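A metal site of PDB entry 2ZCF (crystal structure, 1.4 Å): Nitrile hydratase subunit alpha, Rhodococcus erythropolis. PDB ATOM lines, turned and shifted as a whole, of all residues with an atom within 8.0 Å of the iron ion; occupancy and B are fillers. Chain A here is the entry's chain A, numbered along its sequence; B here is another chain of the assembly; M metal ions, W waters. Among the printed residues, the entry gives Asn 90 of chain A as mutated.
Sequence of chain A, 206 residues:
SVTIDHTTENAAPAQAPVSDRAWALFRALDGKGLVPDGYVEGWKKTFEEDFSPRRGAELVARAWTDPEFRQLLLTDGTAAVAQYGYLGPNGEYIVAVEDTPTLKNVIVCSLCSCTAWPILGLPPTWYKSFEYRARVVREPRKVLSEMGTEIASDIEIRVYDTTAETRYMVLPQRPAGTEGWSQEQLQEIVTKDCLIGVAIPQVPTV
Water W1 lies within hydrogen-bond range of OD1 of CSD 112 (2.7 Å), OG of Ser 113 (2.8 Å) and OD of CSO 114 (2.9 Å).
NH2 of Arg 56 of chain B is in hydrogen-bond range of OD of CSO 114. The side-chain hydroxyl (OH) of Tyr 72 of chain B is in hydrogen-bond range of the side-chain hydroxyl (OG) of Ser 113 (2.6 Å). The backbone carbonyl oxygen (O) of Thr 162 lies close to the side-chain sulfur (SG) of Cys 109 (3.6 Å). The guanidinium group of Arg 56 of chain B lies within salt-bridge range of OD1 of CSD 112 (2.9 Å). OD of CSO 114 sits at hydrogen-bond distance from the guanidinium group (NH2) of Arg 167 (3.5 Å). OH of Tyr 127 sits at hydrogen-bond distance from N of Cys 109 (3.4 Å). OD2 of CSD 112 lies within salt-bridge range of the guanidinium group of Arg 141 of chain B. SG of CSO 114 lies close to the guanidinium group (NH2) of Arg 141 of chain B (3.7 Å).
Along chain A the residues within 4 Å of the iron ion span positions 109 to 114. The nearest printed residue that does not touch the iron ion is Arg 141 of chain B (4.8 Å).
The iron ion is bound by water W1 (2.0 Å), N of CSO 114 (2.0 Å), the backbone nitrogen (N) of Ser 113 (2.0 Å), SG of CSD 112 (2.2 Å), SG of CSO 114 (2.3 Å) and the side-chain sulfur (SG) of Cys 109 (2.3 Å).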
ATOM      1  N   ASN A  90     -35.516 -11.157  31.749  1.00  0.00           N
ATOM      2  CA  ASN A  90     -34.410 -12.112  31.827  1.00  0.00           C
ATOM      3  C   ASN A  90     -33.615 -11.910  33.111  1.00  0.00           C
ATOM      4  O   ASN A  90     -32.418 -12.085  33.252  1.00  0.00           O
ATOM      5  CB  ASN A  90     -33.483 -12.050  30.624  1.00  0.00           C
ATOM      6  CG  ASN A  90     -34.131 -12.811  29.467  1.00  0.00           C
ATOM      7  OD1 ASN A  90     -34.431 -13.996  29.661  1.00  0.00           O
ATOM      8  ND2 ASN A  90     -34.381 -12.164  28.341  1.00  0.00           N
ATOM      9  N   VAL A 108     -23.168 -20.377  31.471  1.00  0.00           N
ATOM     10  CA  VAL A 108     -23.302 -20.412  30.004  1.00  0.00           C
ATOM     11  C   VAL A 108     -24.768 -20.574  29.664  1.00  0.00           C
ATOM     12  O   VAL A 108     -25.571 -20.975  30.514  1.00  0.00           O
ATOM     13  CB  VAL A 108     -22.451 -21.526  29.371  1.00  0.00           C
ATOM     14  CG1 VAL A 108     -22.940 -22.892  29.866  1.00  0.00           C
ATOM     15  CG2 VAL A 108     -22.438 -21.515  27.846  1.00  0.00           C
ATOM     16  N   CYS A 109     -25.146 -20.339  28.404  1.00  0.00           N
ATOM     17  CA  CYS A 109     -26.364 -20.841  27.830  1.00  0.00           C
ATOM     18  C   CYS A 109     -25.978 -21.685  26.601  1.00  0.00           C
ATOM     19  O   CYS A 109     -25.759 -21.152  25.504  1.00  0.00           O
ATOM     20  CB  CYS A 109     -27.333 -19.732  27.424  1.00  0.00           C
ATOM     21  SG  CYS A 109     -28.849 -20.332  26.653  1.00  0.00           S
ATOM     22  N   SER A 110     -25.809 -23.002  26.792  1.00  0.00           N
ATOM     23  CA  SER A 110     -25.320 -23.768  25.627  1.00  0.00           C
ATOM     24  C   SER A 110     -26.333 -23.762  24.494  1.00  0.00           C
ATOM     25  O   SER A 110     -25.908 -23.934  23.349  1.00  0.00           O
ATOM     26  CB  SER A 110     -25.051 -25.211  26.051  1.00  0.00           C
ATOM     27  OG  SER A 110     -26.228 -25.935  26.325  1.00  0.00           O
ATOM     28  N   LEU A 111     -27.632 -23.591  24.771  1.00  0.00           N
ATOM     29  CA  LEU A 111     -28.622 -23.684  23.704  1.00  0.00           C
ATOM     30  C   LEU A 111     -28.882 -22.374  22.987  1.00  0.00           C
ATOM     31  O   LEU A 111     -29.574 -22.424  21.959  1.00  0.00           O
ATOM     32  CB  LEU A 111     -29.932 -24.189  24.351  1.00  0.00           C
ATOM     33  CG  LEU A 111     -29.875 -25.625  24.869  1.00  0.00           C
ATOM     34  CD1 LEU A 111     -31.149 -25.921  25.666  1.00  0.00           C
ATOM     35  CD2 LEU A 111     -29.711 -26.633  23.746  1.00  0.00           C
ATOM     36  N   CSD A 112     -28.376 -21.226  23.495  1.00  0.00           N
ATOM     37  CA  CSD A 112     -28.638 -19.903  22.878  1.00  0.00           C
ATOM     38  CB  CSD A 112     -30.134 -19.546  22.796  1.00  0.00           C
ATOM     39  SG  CSD A 112     -31.008 -19.742  24.357  1.00  0.00           S
ATOM     40  C   CSD A 112     -27.827 -18.773  23.540  1.00  0.00           C
ATOM     41  O   CSD A 112     -26.715 -18.574  23.036  1.00  0.00           O
ATOM     42  OD1 CSD A 112     -32.319 -19.199  24.108  1.00  0.00           O
ATOM     43  OD2 CSD A 112     -31.112 -21.213  24.722  1.00  0.00           O
ATOM     44  N   SER A 113     -28.300 -18.073  24.569  1.00  0.00           N
ATOM     45  CA  SER A 113     -27.499 -16.951  25.061  1.00  0.00           C
ATOM     46  C   SER A 113     -27.980 -16.497  26.448  1.00  0.00           C
ATOM     47  O   SER A 113     -27.453 -15.482  26.914  1.00  0.00           O
ATOM     48  CB  SER A 113     -27.569 -15.765  24.111  1.00  0.00           C
ATOM     49  OG  SER A 113     -28.930 -15.299  24.118  1.00  0.00           O
ATOM     50  N   CSO A 114     -28.942 -17.225  27.009  1.00  0.00           N
ATOM     51  CA  CSO A 114     -29.627 -16.863  28.232  1.00  0.00           C
ATOM     52  CB  CSO A 114     -30.360 -18.100  28.761  1.00  0.00           C
ATOM     53  SG  CSO A 114     -31.387 -18.828  27.431  1.00  0.00           S
ATOM     54  C   CSO A 114     -28.632 -16.368  29.273  1.00  0.00           C
ATOM     55  O   CSO A 114     -27.605 -16.984  29.601  1.00  0.00           O
ATOM     56  OD  CSO A 114     -32.557 -17.841  27.265  1.00  0.00           O
ATOM     57  N   THR A 115     -28.937 -15.208  29.828  1.00  0.00           N
ATOM     58  CA  THR A 115     -28.131 -14.317  30.624  1.00  0.00           C
ATOM     59  C   THR A 115     -29.003 -13.450  31.552  1.00  0.00           C
ATOM     60  O   THR A 115     -30.074 -13.037  31.107  1.00  0.00           O
ATOM     61  CB  THR A 115     -27.374 -13.380  29.681  1.00  0.00           C
ATOM     62  OG1 THR A 115     -26.349 -14.155  28.976  1.00  0.00           O
ATOM     63  CG2 THR A 115     -26.623 -12.285  30.407  1.00  0.00           C
ATOM     64  N   TRP A 117     -29.813 -10.490  32.169  1.00  0.00           N
ATOM     65  CA  TRP A 117     -29.646  -9.187  31.549  1.00  0.00           C
ATOM     66  C   TRP A 117     -29.588  -7.993  32.503  1.00  0.00           C
ATOM     67  O   TRP A 117     -28.677  -7.184  32.344  1.00  0.00           O
ATOM     68  CB  TRP A 117     -30.818  -8.919  30.595  1.00  0.00           C
ATOM     69  CG  TRP A 117     -30.809  -9.735  29.333  1.00  0.00           C
ATOM     70  CD1 TRP A 117     -29.903 -10.653  28.856  1.00  0.00           C
ATOM     71  CD2 TRP A 117     -31.848  -9.649  28.348  1.00  0.00           C
ATOM     72  NE1 TRP A 117     -30.351 -11.133  27.634  1.00  0.00           N
ATOM     73  CE2 TRP A 117     -31.530 -10.527  27.297  1.00  0.00           C
ATOM     74  CE3 TRP A 117     -33.027  -8.882  28.275  1.00  0.00           C
ATOM     75  CZ2 TRP A 117     -32.380 -10.654  26.191  1.00  0.00           C
ATOM     76  CZ3 TRP A 117     -33.865  -8.999  27.183  1.00  0.00           C
ATOM     77  CH2 TRP A 117     -33.531  -9.887  26.156  1.00  0.00           C
ATOM     78  N   PRO A 123     -25.622 -10.258  26.935  1.00  0.00           N
ATOM     79  CA  PRO A 123     -24.393 -11.064  26.822  1.00  0.00           C
ATOM     80  C   PRO A 123     -23.450 -10.507  25.776  1.00  0.00           C
ATOM     81  O   PRO A 123     -23.932  -9.966  24.753  1.00  0.00           O
ATOM     82  CB  PRO A 123     -24.930 -12.427  26.377  1.00  0.00           C
ATOM     83  CG  PRO A 123     -26.291 -12.165  25.814  1.00  0.00           C
ATOM     84  CD  PRO A 123     -26.833 -10.970  26.572  1.00  0.00           C
ATOM     85  N   TYR A 127     -19.772 -14.779  24.466  1.00  0.00           N
ATOM     86  CA  TYR A 127     -20.566 -15.721  25.262  1.00  0.00           C
ATOM     87  C   TYR A 127     -21.591 -16.462  24.399  1.00  0.00           C
ATOM     88  O   TYR A 127     -21.969 -17.591  24.744  1.00  0.00           O
ATOM     89  CB  TYR A 127     -21.275 -14.966  26.341  1.00  0.00           C
ATOM     90  CG  TYR A 127     -22.247 -15.600  27.285  1.00  0.00           C
ATOM     91  CD1 TYR A 127     -23.569 -15.738  26.980  1.00  0.00           C
ATOM     92  CD2 TYR A 127     -21.763 -16.059  28.522  1.00  0.00           C
ATOM     93  CE1 TYR A 127     -24.447 -16.334  27.873  1.00  0.00           C
ATOM     94  CE2 TYR A 127     -22.633 -16.643  29.415  1.00  0.00           C
ATOM     95  CZ  TYR A 127     -23.970 -16.788  29.084  1.00  0.00           C
ATOM     96  OH  TYR A 127     -24.870 -17.344  29.982  1.00  0.00           O
ATOM     97  N   LYS A 128     -21.994 -15.780  23.338  1.00  0.00           N
ATOM     98  CA  LYS A 128     -22.942 -16.354  22.390  1.00  0.00           C
ATOM     99  C   LYS A 128     -22.231 -17.154  21.296  1.00  0.00           C
ATOM    100  O   LYS A 128     -22.898 -17.715  20.454  1.00  0.00           O
ATOM    101  CB  LYS A 128     -23.762 -15.213  21.796  1.00  0.00           C
ATOM    102  CG  LYS A 128     -24.573 -14.475  22.871  1.00  0.00           C
ATOM    103  CD  LYS A 128     -25.303 -13.291  22.302  1.00  0.00           C
ATOM    104  CE  LYS A 128     -24.409 -12.100  22.061  1.00  0.00           C
ATOM    105  NZ  LYS A 128     -25.146 -10.865  21.644  1.00  0.00           N
ATOM    106  N   ARG A 133     -20.301 -21.977  23.746  1.00  0.00           N
ATOM    107  CA  ARG A 133     -21.467 -22.820  23.930  1.00  0.00           C
ATOM    108  C   ARG A 133     -21.132 -24.308  23.805  1.00  0.00           C
ATOM    109  O   ARG A 133     -21.743 -25.120  24.494  1.00  0.00           O
ATOM    110  CB  ARG A 133     -22.520 -22.404  22.898  1.00  0.00           C
ATOM    111  CG  ARG A 133     -23.123 -21.030  23.240  1.00  0.00           C
ATOM    112  CD  ARG A 133     -24.138 -20.561  22.213  1.00  0.00           C
ATOM    113  NE  ARG A 133     -25.065 -21.647  21.884  1.00  0.00           N
ATOM    114  CZ  ARG A 133     -25.776 -21.755  20.777  1.00  0.00           C
ATOM    115  NH1 ARG A 133     -25.743 -20.824  19.815  1.00  0.00           N
ATOM    116  NH2 ARG A 133     -26.541 -22.839  20.625  1.00  0.00           N
ATOM    117  N   ASP A 161     -25.543 -24.349  33.239  1.00  0.00           N
ATOM    118  CA  ASP A 161     -26.147 -24.186  31.914  1.00  0.00           C
ATOM    119  C   ASP A 161     -27.531 -23.590  32.091  1.00  0.00           C
ATOM    120  O   ASP A 161     -28.401 -24.217  32.708  1.00  0.00           O
ATOM    121  CB  ASP A 161     -26.188 -25.554  31.196  1.00  0.00           C
ATOM    122  CG  ASP A 161     -26.364 -25.350  29.699  1.00  0.00           C
ATOM    123  OD1 ASP A 161     -26.627 -24.233  29.235  1.00  0.00           O
ATOM    124  OD2 ASP A 161     -26.230 -26.376  28.970  1.00  0.00           O
ATOM    125  N   THR A 162     -27.734 -22.371  31.573  1.00  0.00           N
ATOM    126  CA  THR A 162     -28.959 -21.615  31.782  1.00  0.00           C
ATOM    127  C   THR A 162     -30.011 -22.113  30.794  1.00  0.00           C
ATOM    128  O   THR A 162     -30.219 -21.501  29.732  1.00  0.00           O
ATOM    129  CB  THR A 162     -28.647 -20.107  31.585  1.00  0.00           C
ATOM    130  OG1 THR A 162     -27.528 -19.725  32.429  1.00  0.00           O
ATOM    131  CG2 THR A 162     -29.857 -19.271  31.981  1.00  0.00           C
ATOM    132  N   THR A 163     -30.680 -23.204  31.142  1.00  0.00           N
ATOM    133  CA  THR A 163     -31.613 -23.862  30.243  1.00  0.00           C
ATOM    134  C   THR A 163     -33.091 -23.599  30.490  1.00  0.00           C
ATOM    135  O   THR A 163     -33.929 -24.053  29.738  1.00  0.00           O
ATOM    136  CB  THR A 163     -31.413 -25.398  30.306  1.00  0.00           C
ATOM    137  OG1 THR A 163     -31.327 -25.802  31.692  1.00  0.00           O
ATOM    138  CG2 THR A 163     -30.070 -25.779  29.669  1.00  0.00           C
ATOM    139  N   ALA A 164     -33.389 -22.834  31.591  1.00  0.00           N
ATOM    140  CA  ALA A 164     -34.810 -22.567  31.844  1.00  0.00           C
ATOM    141  C   ALA A 164     -34.996 -21.119  32.247  1.00  0.00           C
ATOM    142  O   ALA A 164     -34.497 -20.259  31.517  1.00  0.00           O
ATOM    143  CB  ALA A 164     -35.355 -23.557  32.866  1.00  0.00           C
ATOM    144  N   ARG A 167     -31.921 -17.302  36.239  1.00  0.00           N
ATOM    145  CA  ARG A 167     -30.888 -16.449  35.708  1.00  0.00           C
ATOM    146  C   ARG A 167     -29.839 -16.302  36.803  1.00  0.00           C
ATOM    147  O   ARG A 167     -30.158 -15.996  37.954  1.00  0.00           O
ATOM    148  CB  ARG A 167     -31.439 -15.109  35.231  1.00  0.00           C
ATOM    149  CG  ARG A 167     -32.340 -15.324  34.021  1.00  0.00           C
ATOM    150  CD  ARG A 167     -31.543 -15.686  32.757  1.00  0.00           C
ATOM    151  NE  ARG A 167     -32.458 -15.779  31.624  1.00  0.00           N
ATOM    152  CZ  ARG A 167     -33.179 -16.871  31.345  1.00  0.00           C
ATOM    153  NH1 ARG A 167     -33.045 -17.961  32.105  1.00  0.00           N
ATOM    154  NH2 ARG A 167     -33.983 -16.806  30.286  1.00  0.00           N
ATOM    155  N   TYR B  37     -34.377  -8.017  19.353  1.00  0.00           N
ATOM    156  CA  TYR B  37     -34.968  -8.187  20.686  1.00  0.00           C
ATOM    157  C   TYR B  37     -36.179  -7.272  20.886  1.00  0.00           C
ATOM    158  O   TYR B  37     -37.143  -7.675  21.530  1.00  0.00           O
ATOM    159  CB  TYR B  37     -33.900  -7.867  21.729  1.00  0.00           C
ATOM    160  CG  TYR B  37     -32.843  -8.893  22.056  1.00  0.00           C
ATOM    161  CD1 TYR B  37     -32.818 -10.149  21.441  1.00  0.00           C
ATOM    162  CD2 TYR B  37     -31.874  -8.587  22.999  1.00  0.00           C
ATOM    163  CE1 TYR B  37     -31.836 -11.075  21.761  1.00  0.00           C
ATOM    164  CE2 TYR B  37     -30.902  -9.515  23.330  1.00  0.00           C
ATOM    165  CZ  TYR B  37     -30.895 -10.751  22.701  1.00  0.00           C
ATOM    166  OH  TYR B  37     -29.859 -11.556  23.145  1.00  0.00           O
ATOM    167  N   ARG B  56     -37.302 -19.038  20.634  1.00  0.00           N
ATOM    168  CA  ARG B  56     -36.195 -19.985  20.735  1.00  0.00           C
ATOM    169  C   ARG B  56     -36.393 -21.082  19.682  1.00  0.00           C
ATOM    170  O   ARG B  56     -35.480 -21.445  18.928  1.00  0.00           O
ATOM    171  CB  ARG B  56     -36.113 -20.631  22.105  1.00  0.00           C
ATOM    172  CG  ARG B  56     -35.768 -19.638  23.225  1.00  0.00           C
ATOM    173  CD  ARG B  56     -35.282 -20.385  24.475  1.00  0.00           C
ATOM    174  NE  ARG B  56     -34.909 -19.379  25.484  1.00  0.00           N
ATOM    175  CZ  ARG B  56     -35.813 -18.875  26.340  1.00  0.00           C
ATOM    176  NH1 ARG B  56     -37.072 -19.256  26.343  1.00  0.00           N
ATOM    177  NH2 ARG B  56     -35.410 -17.952  27.215  1.00  0.00           N
ATOM    178  N   TYR B  72     -25.354 -14.163  15.579  1.00  0.00           N
ATOM    179  CA  TYR B  72     -26.429 -14.262  16.574  1.00  0.00           C
ATOM    180  C   TYR B  72     -27.613 -13.345  16.304  1.00  0.00           C
ATOM    181  O   TYR B  72     -28.778 -13.758  16.184  1.00  0.00           O
ATOM    182  CB  TYR B  72     -25.770 -13.941  17.954  1.00  0.00           C
ATOM    183  CG  TYR B  72     -26.828 -13.904  19.048  1.00  0.00           C
ATOM    184  CD1 TYR B  72     -27.239 -15.079  19.671  1.00  0.00           C
ATOM    185  CD2 TYR B  72     -27.438 -12.709  19.482  1.00  0.00           C
ATOM    186  CE1 TYR B  72     -28.181 -15.096  20.670  1.00  0.00           C
ATOM    187  CE2 TYR B  72     -28.413 -12.747  20.465  1.00  0.00           C
ATOM    188  CZ  TYR B  72     -28.794 -13.900  21.061  1.00  0.00           C
ATOM    189  OH  TYR B  72     -29.762 -13.926  22.043  1.00  0.00           O
ATOM    190  N   TYR B  76     -32.024 -13.912  15.139  1.00  0.00           N
ATOM    191  CA  TYR B  76     -33.295 -13.454  15.730  1.00  0.00           C
ATOM    192  C   TYR B  76     -34.087 -12.545  14.806  1.00  0.00           C
ATOM    193  O   TYR B  76     -35.330 -12.571  14.855  1.00  0.00           O
ATOM    194  CB  TYR B  76     -33.026 -12.758  17.092  1.00  0.00           C
ATOM    195  CG  TYR B  76     -32.595 -13.929  17.998  1.00  0.00           C
ATOM    196  CD1 TYR B  76     -33.504 -14.679  18.725  1.00  0.00           C
ATOM    197  CD2 TYR B  76     -31.230 -14.244  17.999  1.00  0.00           C
ATOM    198  CE1 TYR B  76     -33.064 -15.750  19.518  1.00  0.00           C
ATOM    199  CE2 TYR B  76     -30.851 -15.301  18.775  1.00  0.00           C
ATOM    200  CZ  TYR B  76     -31.721 -16.042  19.522  1.00  0.00           C
ATOM    201  OH  TYR B  76     -31.201 -17.091  20.257  1.00  0.00           O
ATOM    202  N   ARG B 141     -36.186 -27.949  26.358  1.00  0.00           N
ATOM    203  CA  ARG B 141     -35.097 -27.248  27.039  1.00  0.00           C
ATOM    204  C   ARG B 141     -34.236 -28.198  27.854  1.00  0.00           C
ATOM    205  O   ARG B 141     -33.829 -28.049  28.989  1.00  0.00           O
ATOM    206  CB  ARG B 141     -35.666 -26.149  27.953  1.00  0.00           C
ATOM    207  CG  ARG B 141     -36.343 -25.068  27.120  1.00  0.00           C
ATOM    208  CD  ARG B 141     -35.357 -24.418  26.152  1.00  0.00           C
ATOM    209  NE  ARG B 141     -34.309 -23.680  26.889  1.00  0.00           N
ATOM    210  CZ  ARG B 141     -33.319 -23.039  26.261  1.00  0.00           C
ATOM    211  NH1 ARG B 141     -33.232 -23.113  24.933  1.00  0.00           N
ATOM    212  NH2 ARG B 141     -32.417 -22.350  26.936  1.00  0.00           N
HETATM  213 FE    FE M   1     -29.897 -18.474  25.751  1.00  0.00          FE
HETATM  214  O   HOH W   1     -30.945 -16.993  25.003  1.00  0.00           O
